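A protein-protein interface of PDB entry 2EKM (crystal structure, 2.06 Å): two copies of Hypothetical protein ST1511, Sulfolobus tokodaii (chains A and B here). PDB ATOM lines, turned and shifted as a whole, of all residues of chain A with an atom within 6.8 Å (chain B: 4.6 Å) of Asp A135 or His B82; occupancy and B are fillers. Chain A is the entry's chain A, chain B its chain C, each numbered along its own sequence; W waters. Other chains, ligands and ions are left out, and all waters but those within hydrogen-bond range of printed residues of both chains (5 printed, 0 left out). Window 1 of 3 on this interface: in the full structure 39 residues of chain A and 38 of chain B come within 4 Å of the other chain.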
ATOM      1  N   PHE A 110       7.361  -8.121 -24.383  1.00  0.00           N
ATOM      2  CA  PHE A 110       8.084  -6.854 -24.434  1.00  0.00           C
ATOM      3  C   PHE A 110       7.397  -5.719 -23.668  1.00  0.00           C
ATOM      4  O   PHE A 110       8.069  -4.857 -23.095  1.00  0.00           O
ATOM      5  CB  PHE A 110       8.290  -6.417 -25.894  1.00  0.00           C
ATOM      6  CG  PHE A 110       9.139  -7.369 -26.712  1.00  0.00           C
ATOM      7  CD1 PHE A 110      10.451  -7.649 -26.345  1.00  0.00           C
ATOM      8  CD2 PHE A 110       8.628  -7.960 -27.864  1.00  0.00           C
ATOM      9  CE1 PHE A 110      11.250  -8.509 -27.119  1.00  0.00           C
ATOM     10  CE2 PHE A 110       9.411  -8.816 -28.642  1.00  0.00           C
ATOM     11  CZ  PHE A 110      10.725  -9.091 -28.269  1.00  0.00           C
ATOM     12  N   ALA A 111       6.069  -5.715 -23.658  1.00  0.00           N
ATOM     13  CA  ALA A 111       5.345  -4.660 -22.969  1.00  0.00           C
ATOM     14  C   ALA A 111       3.870  -4.974 -22.761  1.00  0.00           C
ATOM     15  O   ALA A 111       3.271  -5.742 -23.509  1.00  0.00           O
ATOM     16  CB  ALA A 111       5.483  -3.346 -23.750  1.00  0.00           C
ATOM     17  N   ALA A 112       3.308  -4.361 -21.728  1.00  0.00           N
ATOM     18  CA  ALA A 112       1.894  -4.479 -21.376  1.00  0.00           C
ATOM     19  C   ALA A 112       1.608  -3.084 -20.829  1.00  0.00           C
ATOM     20  O   ALA A 112       2.070  -2.741 -19.738  1.00  0.00           O
ATOM     21  CB  ALA A 112       1.698  -5.530 -20.295  1.00  0.00           C
ATOM     22  N   THR A 113       0.864  -2.273 -21.575  1.00  0.00           N
ATOM     23  CA  THR A 113       0.625  -0.907 -21.130  1.00  0.00           C
ATOM     24  C   THR A 113      -0.483  -0.173 -21.885  1.00  0.00           C
ATOM     25  O   THR A 113      -0.978  -0.642 -22.911  1.00  0.00           O
ATOM     26  CB  THR A 113       1.929  -0.084 -21.290  1.00  0.00           C
ATOM     27  OG1 THR A 113       1.802   1.180 -20.634  1.00  0.00           O
ATOM     28  CG2 THR A 113       2.213   0.157 -22.775  1.00  0.00           C
ATOM     29  N   ALA A 114      -0.855   0.990 -21.355  1.00  0.00           N
ATOM     30  CA  ALA A 114      -1.858   1.856 -21.961  1.00  0.00           C
ATOM     31  C   ALA A 114      -1.200   3.222 -22.163  1.00  0.00           C
ATOM     32  O   ALA A 114      -1.794   4.133 -22.735  1.00  0.00           O
ATOM     33  CB  ALA A 114      -3.078   1.983 -21.052  1.00  0.00           C
ATOM     34  N   ASN A 115       0.034   3.346 -21.678  1.00  0.00           N
ATOM     35  CA  ASN A 115       0.812   4.579 -21.792  1.00  0.00           C
ATOM     36  C   ASN A 115       1.338   4.689 -23.225  1.00  0.00           C
ATOM     37  O   ASN A 115       1.406   3.717 -23.966  1.00  0.00           O
ATOM     38  CB  ASN A 115       2.017   4.531 -20.851  1.00  0.00           C
ATOM     39  CG  ASN A 115       1.625   4.573 -19.392  1.00  0.00           C
ATOM     40  OD1 ASN A 115       2.294   3.984 -18.545  1.00  0.00           O
ATOM     41  ND2 ASN A 115       0.549   5.285 -19.086  1.00  0.00           N
ATOM     42  N   PRO A 116       1.648   5.949 -23.576  1.00  0.00           N
ATOM     43  CA  PRO A 116       2.215   6.161 -24.893  1.00  0.00           C
ATOM     44  C   PRO A 116       3.377   5.174 -25.068  1.00  0.00           C
ATOM     45  O   PRO A 116       4.209   5.059 -24.164  1.00  0.00           O
ATOM     46  CB  PRO A 116       2.732   7.630 -24.896  1.00  0.00           C
ATOM     47  CG  PRO A 116       1.729   8.278 -23.987  1.00  0.00           C
ATOM     48  CD  PRO A 116       1.587   7.261 -22.869  1.00  0.00           C
ATOM     49  N   LEU A 117       3.410   4.435 -26.171  1.00  0.00           N
ATOM     50  CA  LEU A 117       4.429   3.408 -26.334  1.00  0.00           C
ATOM     51  C   LEU A 117       5.167   3.407 -27.663  1.00  0.00           C
ATOM     52  O   LEU A 117       4.569   3.566 -28.726  1.00  0.00           O
ATOM     53  CB  LEU A 117       3.789   2.031 -26.126  1.00  0.00           C
ATOM     54  CG  LEU A 117       4.663   0.783 -26.305  1.00  0.00           C
ATOM     55  CD1 LEU A 117       5.595   0.628 -25.111  1.00  0.00           C
ATOM     56  CD2 LEU A 117       3.765  -0.453 -26.438  1.00  0.00           C
ATOM     57  N   GLN A 118       6.481   3.214 -27.581  1.00  0.00           N
ATOM     58  CA  GLN A 118       7.333   3.138 -28.759  1.00  0.00           C
ATOM     59  C   GLN A 118       8.037   1.783 -28.730  1.00  0.00           C
ATOM     60  O   GLN A 118       8.493   1.335 -27.675  1.00  0.00           O
ATOM     61  CB  GLN A 118       8.397   4.238 -28.740  1.00  0.00           C
ATOM     62  CG  GLN A 118       7.909   5.638 -29.077  1.00  0.00           C
ATOM     63  CD  GLN A 118       9.019   6.667 -28.949  1.00  0.00           C
ATOM     64  OE1 GLN A 118       9.018   7.698 -29.628  1.00  0.00           O
ATOM     65  NE2 GLN A 118       9.973   6.393 -28.067  1.00  0.00           N
ATOM     66  N   VAL A 133      11.473  -1.340 -25.807  1.00  0.00           N
ATOM     67  CA  VAL A 133      10.363  -0.412 -25.942  1.00  0.00           C
ATOM     68  C   VAL A 133      10.568   0.794 -25.033  1.00  0.00           C
ATOM     69  O   VAL A 133      11.349   0.741 -24.085  1.00  0.00           O
ATOM     70  CB  VAL A 133       9.016  -1.063 -25.536  1.00  0.00           C
ATOM     71  CG1 VAL A 133       8.766  -2.328 -26.356  1.00  0.00           C
ATOM     72  CG2 VAL A 133       9.023  -1.387 -24.045  1.00  0.00           C
ATOM     73  N   VAL A 134       9.877   1.884 -25.346  1.00  0.00           N
ATOM     74  CA  VAL A 134       9.919   3.077 -24.515  1.00  0.00           C
ATOM     75  C   VAL A 134       8.491   3.144 -23.996  1.00  0.00           C
ATOM     76  O   VAL A 134       7.576   3.571 -24.701  1.00  0.00           O
ATOM     77  CB  VAL A 134      10.246   4.357 -25.315  1.00  0.00           C
ATOM     78  CG1 VAL A 134      10.270   5.566 -24.372  1.00  0.00           C
ATOM     79  CG2 VAL A 134      11.596   4.207 -26.001  1.00  0.00           C
ATOM     80  N   ASP A 135       8.308   2.675 -22.767  1.00  0.00           N
ATOM     81  CA  ASP A 135       7.000   2.636 -22.133  1.00  0.00           C
ATOM     82  C   ASP A 135       6.807   3.840 -21.219  1.00  0.00           C
ATOM     83  O   ASP A 135       7.350   3.888 -20.118  1.00  0.00           O
ATOM     84  CB  ASP A 135       6.867   1.351 -21.309  1.00  0.00           C
ATOM     85  CG  ASP A 135       5.452   1.115 -20.817  1.00  0.00           C
ATOM     86  OD1 ASP A 135       4.651   2.071 -20.830  1.00  0.00           O
ATOM     87  OD2 ASP A 135       5.148  -0.027 -20.409  1.00  0.00           O
ATOM     88  N   GLY A 136       6.032   4.812 -21.680  1.00  0.00           N
ATOM     89  CA  GLY A 136       5.792   5.983 -20.863  1.00  0.00           C
ATOM     90  C   GLY A 136       6.982   6.915 -20.795  1.00  0.00           C
ATOM     91  O   GLY A 136       7.837   6.924 -21.685  1.00  0.00           O
ATOM     92  N   TYR A 137       7.054   7.682 -19.714  1.00  0.00           N
ATOM     93  CA  TYR A 137       8.116   8.664 -19.555  1.00  0.00           C
ATOM     94  C   TYR A 137       9.139   8.354 -18.471  1.00  0.00           C
ATOM     95  O   TYR A 137       8.980   7.410 -17.694  1.00  0.00           O
ATOM     96  CB  TYR A 137       7.479  10.032 -19.307  1.00  0.00           C
ATOM     97  CG  TYR A 137       6.455  10.395 -20.363  1.00  0.00           C
ATOM     98  CD1 TYR A 137       6.855  10.796 -21.638  1.00  0.00           C
ATOM     99  CD2 TYR A 137       5.088  10.292 -20.106  1.00  0.00           C
ATOM    100  CE1 TYR A 137       5.922  11.082 -22.632  1.00  0.00           C
ATOM    101  CE2 TYR A 137       4.140  10.576 -21.098  1.00  0.00           C
ATOM    102  CZ  TYR A 137       4.567  10.971 -22.358  1.00  0.00           C
ATOM    103  OH  TYR A 137       3.650  11.252 -23.347  1.00  0.00           O
ATOM    104  N   THR A 138      10.189   9.172 -18.430  1.00  0.00           N
ATOM    105  CA  THR A 138      11.271   9.020 -17.465  1.00  0.00           C
ATOM    106  C   THR A 138      10.837   9.519 -16.088  1.00  0.00           C
ATOM    107  O   THR A 138       9.985  10.397 -15.980  1.00  0.00           O
ATOM    108  CB  THR A 138      12.519   9.807 -17.918  1.00  0.00           C
ATOM    109  OG1 THR A 138      12.200  11.203 -17.989  1.00  0.00           O
ATOM    110  CG2 THR A 138      12.978   9.329 -19.298  1.00  0.00           C
ATOM    111  N   GLY B  21      13.870  -5.523 -13.901  1.00  0.00           N
ATOM    112  CA  GLY B  21      12.910  -5.949 -14.901  1.00  0.00           C
ATOM    113  C   GLY B  21      11.983  -4.849 -15.383  1.00  0.00           C
ATOM    114  O   GLY B  21      12.236  -3.658 -15.185  1.00  0.00           O
ATOM    115  N   GLN B  22      10.899  -5.267 -16.024  1.00  0.00           N
ATOM    116  CA  GLN B  22       9.906  -4.350 -16.563  1.00  0.00           C
ATOM    117  C   GLN B  22       8.532  -4.796 -16.082  1.00  0.00           C
ATOM    118  O   GLN B  22       8.252  -5.993 -15.995  1.00  0.00           O
ATOM    119  CB  GLN B  22       9.951  -4.376 -18.089  1.00  0.00           C
ATOM    120  CG  GLN B  22       9.161  -3.271 -18.762  1.00  0.00           C
ATOM    121  CD  GLN B  22       9.169  -3.408 -20.271  1.00  0.00           C
ATOM    122  OE1 GLN B  22      10.224  -3.580 -20.883  1.00  0.00           O
ATOM    123  NE2 GLN B  22       7.992  -3.331 -20.882  1.00  0.00           N
ATOM    124  N   SER B  23       7.674  -3.831 -15.787  1.00  0.00           N
ATOM    125  CA  SER B  23       6.342  -4.128 -15.292  1.00  0.00           C
ATOM    126  C   SER B  23       5.382  -3.046 -15.757  1.00  0.00           C
ATOM    127  O   SER B  23       5.675  -2.295 -16.685  1.00  0.00           O
ATOM    128  CB  SER B  23       6.371  -4.170 -13.761  1.00  0.00           C
ATOM    129  OG  SER B  23       5.162  -4.674 -13.234  1.00  0.00           O
ATOM    130  N   HIS B  24       4.228  -2.974 -15.109  1.00  0.00           N
ATOM    131  CA  HIS B  24       3.237  -1.959 -15.438  1.00  0.00           C
ATOM    132  C   HIS B  24       2.277  -1.884 -14.262  1.00  0.00           C
ATOM    133  O   HIS B  24       2.203  -2.821 -13.468  1.00  0.00           O
ATOM    134  CB  HIS B  24       2.482  -2.326 -16.723  1.00  0.00           C
ATOM    135  CG  HIS B  24       1.394  -3.335 -16.521  1.00  0.00           C
ATOM    136  ND1 HIS B  24       1.644  -4.653 -16.208  1.00  0.00           N
ATOM    137  CD2 HIS B  24       0.047  -3.208 -16.561  1.00  0.00           C
ATOM    138  CE1 HIS B  24       0.497  -5.294 -16.062  1.00  0.00           C
ATOM    139  NE2 HIS B  24      -0.487  -4.439 -16.270  1.00  0.00           N
ATOM    140  N   PHE B  25       1.559  -0.770 -14.150  1.00  0.00           N
ATOM    141  CA  PHE B  25       0.589  -0.555 -13.072  1.00  0.00           C
ATOM    142  C   PHE B  25       1.278  -0.354 -11.722  1.00  0.00           C
ATOM    143  O   PHE B  25       2.159  -1.122 -11.333  1.00  0.00           O
ATOM    144  CB  PHE B  25      -0.388  -1.735 -12.978  1.00  0.00           C
ATOM    145  CG  PHE B  25      -1.607  -1.454 -12.131  1.00  0.00           C
ATOM    146  CD1 PHE B  25      -2.086  -0.152 -11.973  1.00  0.00           C
ATOM    147  CD2 PHE B  25      -2.294  -2.495 -11.512  1.00  0.00           C
ATOM    148  CE1 PHE B  25      -3.230   0.109 -11.211  1.00  0.00           C
ATOM    149  CE2 PHE B  25      -3.441  -2.244 -10.745  1.00  0.00           C
ATOM    150  CZ  PHE B  25      -3.906  -0.941 -10.598  1.00  0.00           C
ATOM    151  N   PHE B  49      10.116   1.156  -8.419  1.00  0.00           N
ATOM    152  CA  PHE B  49       9.369   1.020  -9.668  1.00  0.00           C
ATOM    153  C   PHE B  49       9.167   2.392 -10.302  1.00  0.00           C
ATOM    154  O   PHE B  49       8.736   3.334  -9.633  1.00  0.00           O
ATOM    155  CB  PHE B  49       8.008   0.373  -9.394  1.00  0.00           C
ATOM    156  CG  PHE B  49       7.091   0.348 -10.585  1.00  0.00           C
ATOM    157  CD1 PHE B  49       7.389  -0.430 -11.700  1.00  0.00           C
ATOM    158  CD2 PHE B  49       5.917   1.098 -10.588  1.00  0.00           C
ATOM    159  CE1 PHE B  49       6.523  -0.461 -12.805  1.00  0.00           C
ATOM    160  CE2 PHE B  49       5.046   1.075 -11.687  1.00  0.00           C
ATOM    161  CZ  PHE B  49       5.353   0.293 -12.794  1.00  0.00           C
ATOM    162  N   CYS B  50       9.462   2.496 -11.594  1.00  0.00           N
ATOM    163  CA  CYS B  50       9.325   3.762 -12.306  1.00  0.00           C
ATOM    164  C   CYS B  50       7.947   4.012 -12.897  1.00  0.00           C
ATOM    165  O   CYS B  50       7.624   3.524 -13.982  1.00  0.00           O
ATOM    166  CB  CYS B  50      10.366   3.861 -13.426  1.00  0.00           C
ATOM    167  SG  CYS B  50      12.078   3.903 -12.856  1.00  0.00           S
ATOM    168  N   ALA B  52       5.429   5.391 -15.040  1.00  0.00           N
ATOM    169  CA  ALA B  52       5.644   5.947 -16.374  1.00  0.00           C
ATOM    170  C   ALA B  52       4.752   7.102 -16.813  1.00  0.00           C
ATOM    171  O   ALA B  52       4.982   7.697 -17.869  1.00  0.00           O
ATOM    172  CB  ALA B  52       5.571   4.828 -17.401  1.00  0.00           C
ATOM    173  N   ALA B  80      14.216   4.549 -17.142  1.00  0.00           N
ATOM    174  CA  ALA B  80      13.294   4.087 -18.169  1.00  0.00           C
ATOM    175  C   ALA B  80      11.935   3.797 -17.537  1.00  0.00           C
ATOM    176  O   ALA B  80      11.842   3.077 -16.541  1.00  0.00           O
ATOM    177  CB  ALA B  80      13.845   2.837 -18.844  1.00  0.00           C
ATOM    178  N   GLY B  81      10.889   4.370 -18.120  1.00  0.00           N
ATOM    179  CA  GLY B  81       9.548   4.168 -17.602  1.00  0.00           C
ATOM    180  C   GLY B  81       9.162   2.706 -17.453  1.00  0.00           C
ATOM    181  O   GLY B  81       9.485   1.876 -18.308  1.00  0.00           O
ATOM    182  N   HIS B  82       8.476   2.403 -16.351  1.00  0.00           N
ATOM    183  CA  HIS B  82       8.000   1.056 -16.026  1.00  0.00           C
ATOM    184  C   HIS B  82       9.060   0.021 -15.660  1.00  0.00           C
ATOM    185  O   HIS B  82       8.771  -1.175 -15.554  1.00  0.00           O
ATOM    186  CB  HIS B  82       7.099   0.529 -17.149  1.00  0.00           C
ATOM    187  CG  HIS B  82       5.661   0.926 -16.995  1.00  0.00           C
ATOM    188  ND1 HIS B  82       4.706   0.664 -17.951  1.00  0.00           N
ATOM    189  CD2 HIS B  82       5.013   1.544 -15.977  1.00  0.00           C
ATOM    190  CE1 HIS B  82       3.532   1.102 -17.531  1.00  0.00           C
ATOM    191  NE2 HIS B  82       3.691   1.640 -16.335  1.00  0.00           N
ATOM    192  N   THR B  83      10.285   0.485 -15.450  1.00  0.00           N
ATOM    193  CA  THR B  83      11.373  -0.395 -15.052  1.00  0.00           C
ATOM    194  C   THR B  83      11.241  -0.604 -13.547  1.00  0.00           C
ATOM    195  O   THR B  83      10.783   0.289 -12.839  1.00  0.00           O
ATOM    196  CB  THR B  83      12.761   0.258 -15.291  1.00  0.00           C
ATOM    197  OG1 THR B  83      12.943   0.522 -16.685  1.00  0.00           O
ATOM    198  CG2 THR B  83      13.876  -0.668 -14.802  1.00  0.00           C
ATOM    199  N   PHE B  84      11.620  -1.780 -13.055  1.00  0.00           N
ATOM    200  CA  PHE B  84      11.585  -2.012 -11.617  1.00  0.00           C
ATOM    201  C   PHE B  84      12.936  -2.579 -11.208  1.00  0.00           C
ATOM    202  O   PHE B  84      13.580  -3.281 -11.987  1.00  0.00           O
ATOM    203  CB  PHE B  84      10.419  -2.936 -11.203  1.00  0.00           C
ATOM    204  CG  PHE B  84      10.586  -4.385 -11.590  1.00  0.00           C
ATOM    205  CD1 PHE B  84      11.355  -5.246 -10.813  1.00  0.00           C
ATOM    206  CD2 PHE B  84       9.925  -4.899 -12.706  1.00  0.00           C
ATOM    207  CE1 PHE B  84      11.462  -6.603 -11.134  1.00  0.00           C
ATOM    208  CE2 PHE B  84      10.024  -6.252 -13.041  1.00  0.00           C
ATOM    209  CZ  PHE B  84      10.794  -7.107 -12.251  1.00  0.00           C
ATOM    210  N   GLN B 126      10.632  10.579 -26.832  1.00  0.00           N
ATOM    211  CA  GLN B 126       9.626  10.365 -25.795  1.00  0.00           C
ATOM    212  C   GLN B 126      10.242  10.085 -24.429  1.00  0.00           C
ATOM    213  O   GLN B 126       9.852  10.681 -23.428  1.00  0.00           O
ATOM    214  CB  GLN B 126       8.708   9.197 -26.160  1.00  0.00           C
ATOM    215  CG  GLN B 126       7.652   8.908 -25.104  1.00  0.00           C
ATOM    216  CD  GLN B 126       6.801   7.701 -25.451  1.00  0.00           C
ATOM    217  OE1 GLN B 126       6.234   7.621 -26.540  1.00  0.00           O
ATOM    218  NE2 GLN B 126       6.704   6.756 -24.521  1.00  0.00           N
HETATM  219  O   HOH W   1       5.331  -2.653 -20.008  1.00  0.00           O
HETATM  220  O   HOH W   2      10.673   2.460 -20.965  1.00  0.00           O
HETATM  221  O   HOH W   3      10.188  11.108 -20.663  1.00  0.00           O
HETATM  222  O   HOH W   4      12.433  -2.230 -23.152  1.00  0.00           O
HETATM  223  O   HOH W   5      10.435   6.139 -20.545  1.00  0.00           O
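Of the 15 printed residues of chain A, 12 touch a printed residue of chain B.
Among the printed residues, no Asp or Glu carboxylate lies within 4 Å of a Lys or Arg side-chain nitrogen of the other chain.
No position is printed for both chains.
Of the 18 pairs that touch across the chains among the printed residues, none has its exchanged pair printed and touching as well.
The backbone NH of Asn A115 lies within hydrogen-bond range of the side-chain hydroxyl of Thr A113 (3.0 Å).
OG1 of Thr A113 sits at hydrogen-bond distance from OD1 of Asp A135.
O of Pro A116 lies within hydrogen-bond range of N of Gly A136 (3.1 Å).
The backbone NH (N) of Val A134 sits at hydrogen-bond distance from the backbone carbonyl oxygen (O) of Gln A118.
The backbone NH (N) of Ser B23 lies within hydrogen-bond range of the backbone carbonyl oxygen (O) of His B82.
N of His B82 is in hydrogen-bond range of O of Cys B50, at 2.8 Å.
Among the printed residues, pairs that only touch across the chains: Ala A111 with Gln B22 (3.6 Å), Ala A112 with His B24 (3.1 Å), Thr A113 with His B82 (3.6 Å), Asn A115 with Ala B52 (3.6 Å), Asn A115 with His B82 (3.3 Å), Gln A118 with Gln B126 (3.6 Å), Val A133 with Gln B22 (3.9 Å), Asp A135 with Ala B52 (3.4 Å), Gly A136 with Ala B52 (3.5 Å), Tyr A137 with Gly B81 (3.3 Å) and Tyr A137 with Gln B126 (3.5 Å).
Printed residues of chain B within 4 Å of Ala A111: Gln B22 (3.6 Å).
Of the printed residues of chain B, Val A133 touches Gln B22 (3.9 Å).
Of chain B, only Ala B52 (3.4 Å), Gly B81 (3.4 Å) and His B82 (2.6 Å) come within 4 Å of Asp A135.
Of the printed residues of chain B, Tyr A137 touches Ala B52, Gly B81 and Gln B126.
Thr A138 touches none of the printed residues of chain B.
Of chain A, only Thr A113 (3.6 Å), Asn A115 (3.3 Å) and Asp A135 (2.6 Å) come within 4 Å of His B82.
Phe B84 touches none of the printed residues of chain A.
The nearest residue of chain A that does not touch His B82 is Ala A112 (4.7 Å).
NE2 of Gln B22 sits at hydrogen-bond distance from O of Phe A110, 2.7 Å away.
The side-chain amide nitrogen (NE2) of Gln B126 sits at hydrogen-bond distance from the backbone carbonyl oxygen (O) of Pro A116.
The side-chain amide nitrogen of Gln B126 is in hydrogen-bond range of the backbone carbonyl oxygen of Val A134, at 3.3 Å.
The side-chain carboxylate (OD2) of Asp A135 sits at hydrogen-bond distance from a ring nitrogen (ND1) of His B82.
The side-chain amide nitrogen (NE2) of Gln B126 lies within hydrogen-bond range of the backbone carbonyl oxygen (O) of Gly A136.
The backbone NH (N) of Tyr A137 is in hydrogen-bond range of the backbone carbonyl oxygen (O) of Ala B52 (2.8 Å).
The backbone carbonyl oxygen (O) of Asp A135 sits close to the backbone carbonyl oxygen (O) of Gly B81, 3.4 Å away.
Water W1 lies within hydrogen-bond range of the side-chain carboxylate (OD2) of Asp A135, the side-chain amide nitrogen (NE2) of Gln B22, the backbone NH (N) of Ala A112 and the backbone carbonyl oxygen (O) of Ser B23.
Water W3 bridges the backbone carbonyl oxygen (O) of Gln B126 (2.8 Å) and the backbone NH (N) of Thr A138 (3.0 Å).
Water W5 lies within hydrogen-bond range of the backbone carbonyl oxygen of Gly A136 (2.9 Å), the backbone NH of Gly B81 (3.0 Å) and the backbone carbonyl oxygen of Tyr A137 (3.4 Å).
Water W4 lies within hydrogen-bond range of N of Val A133 and OE1 of Gln B22.
Water W2 lies within hydrogen-bond range of O of Gly B81 (3.0 Å) and N of Asp A135 (3.0 Å).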
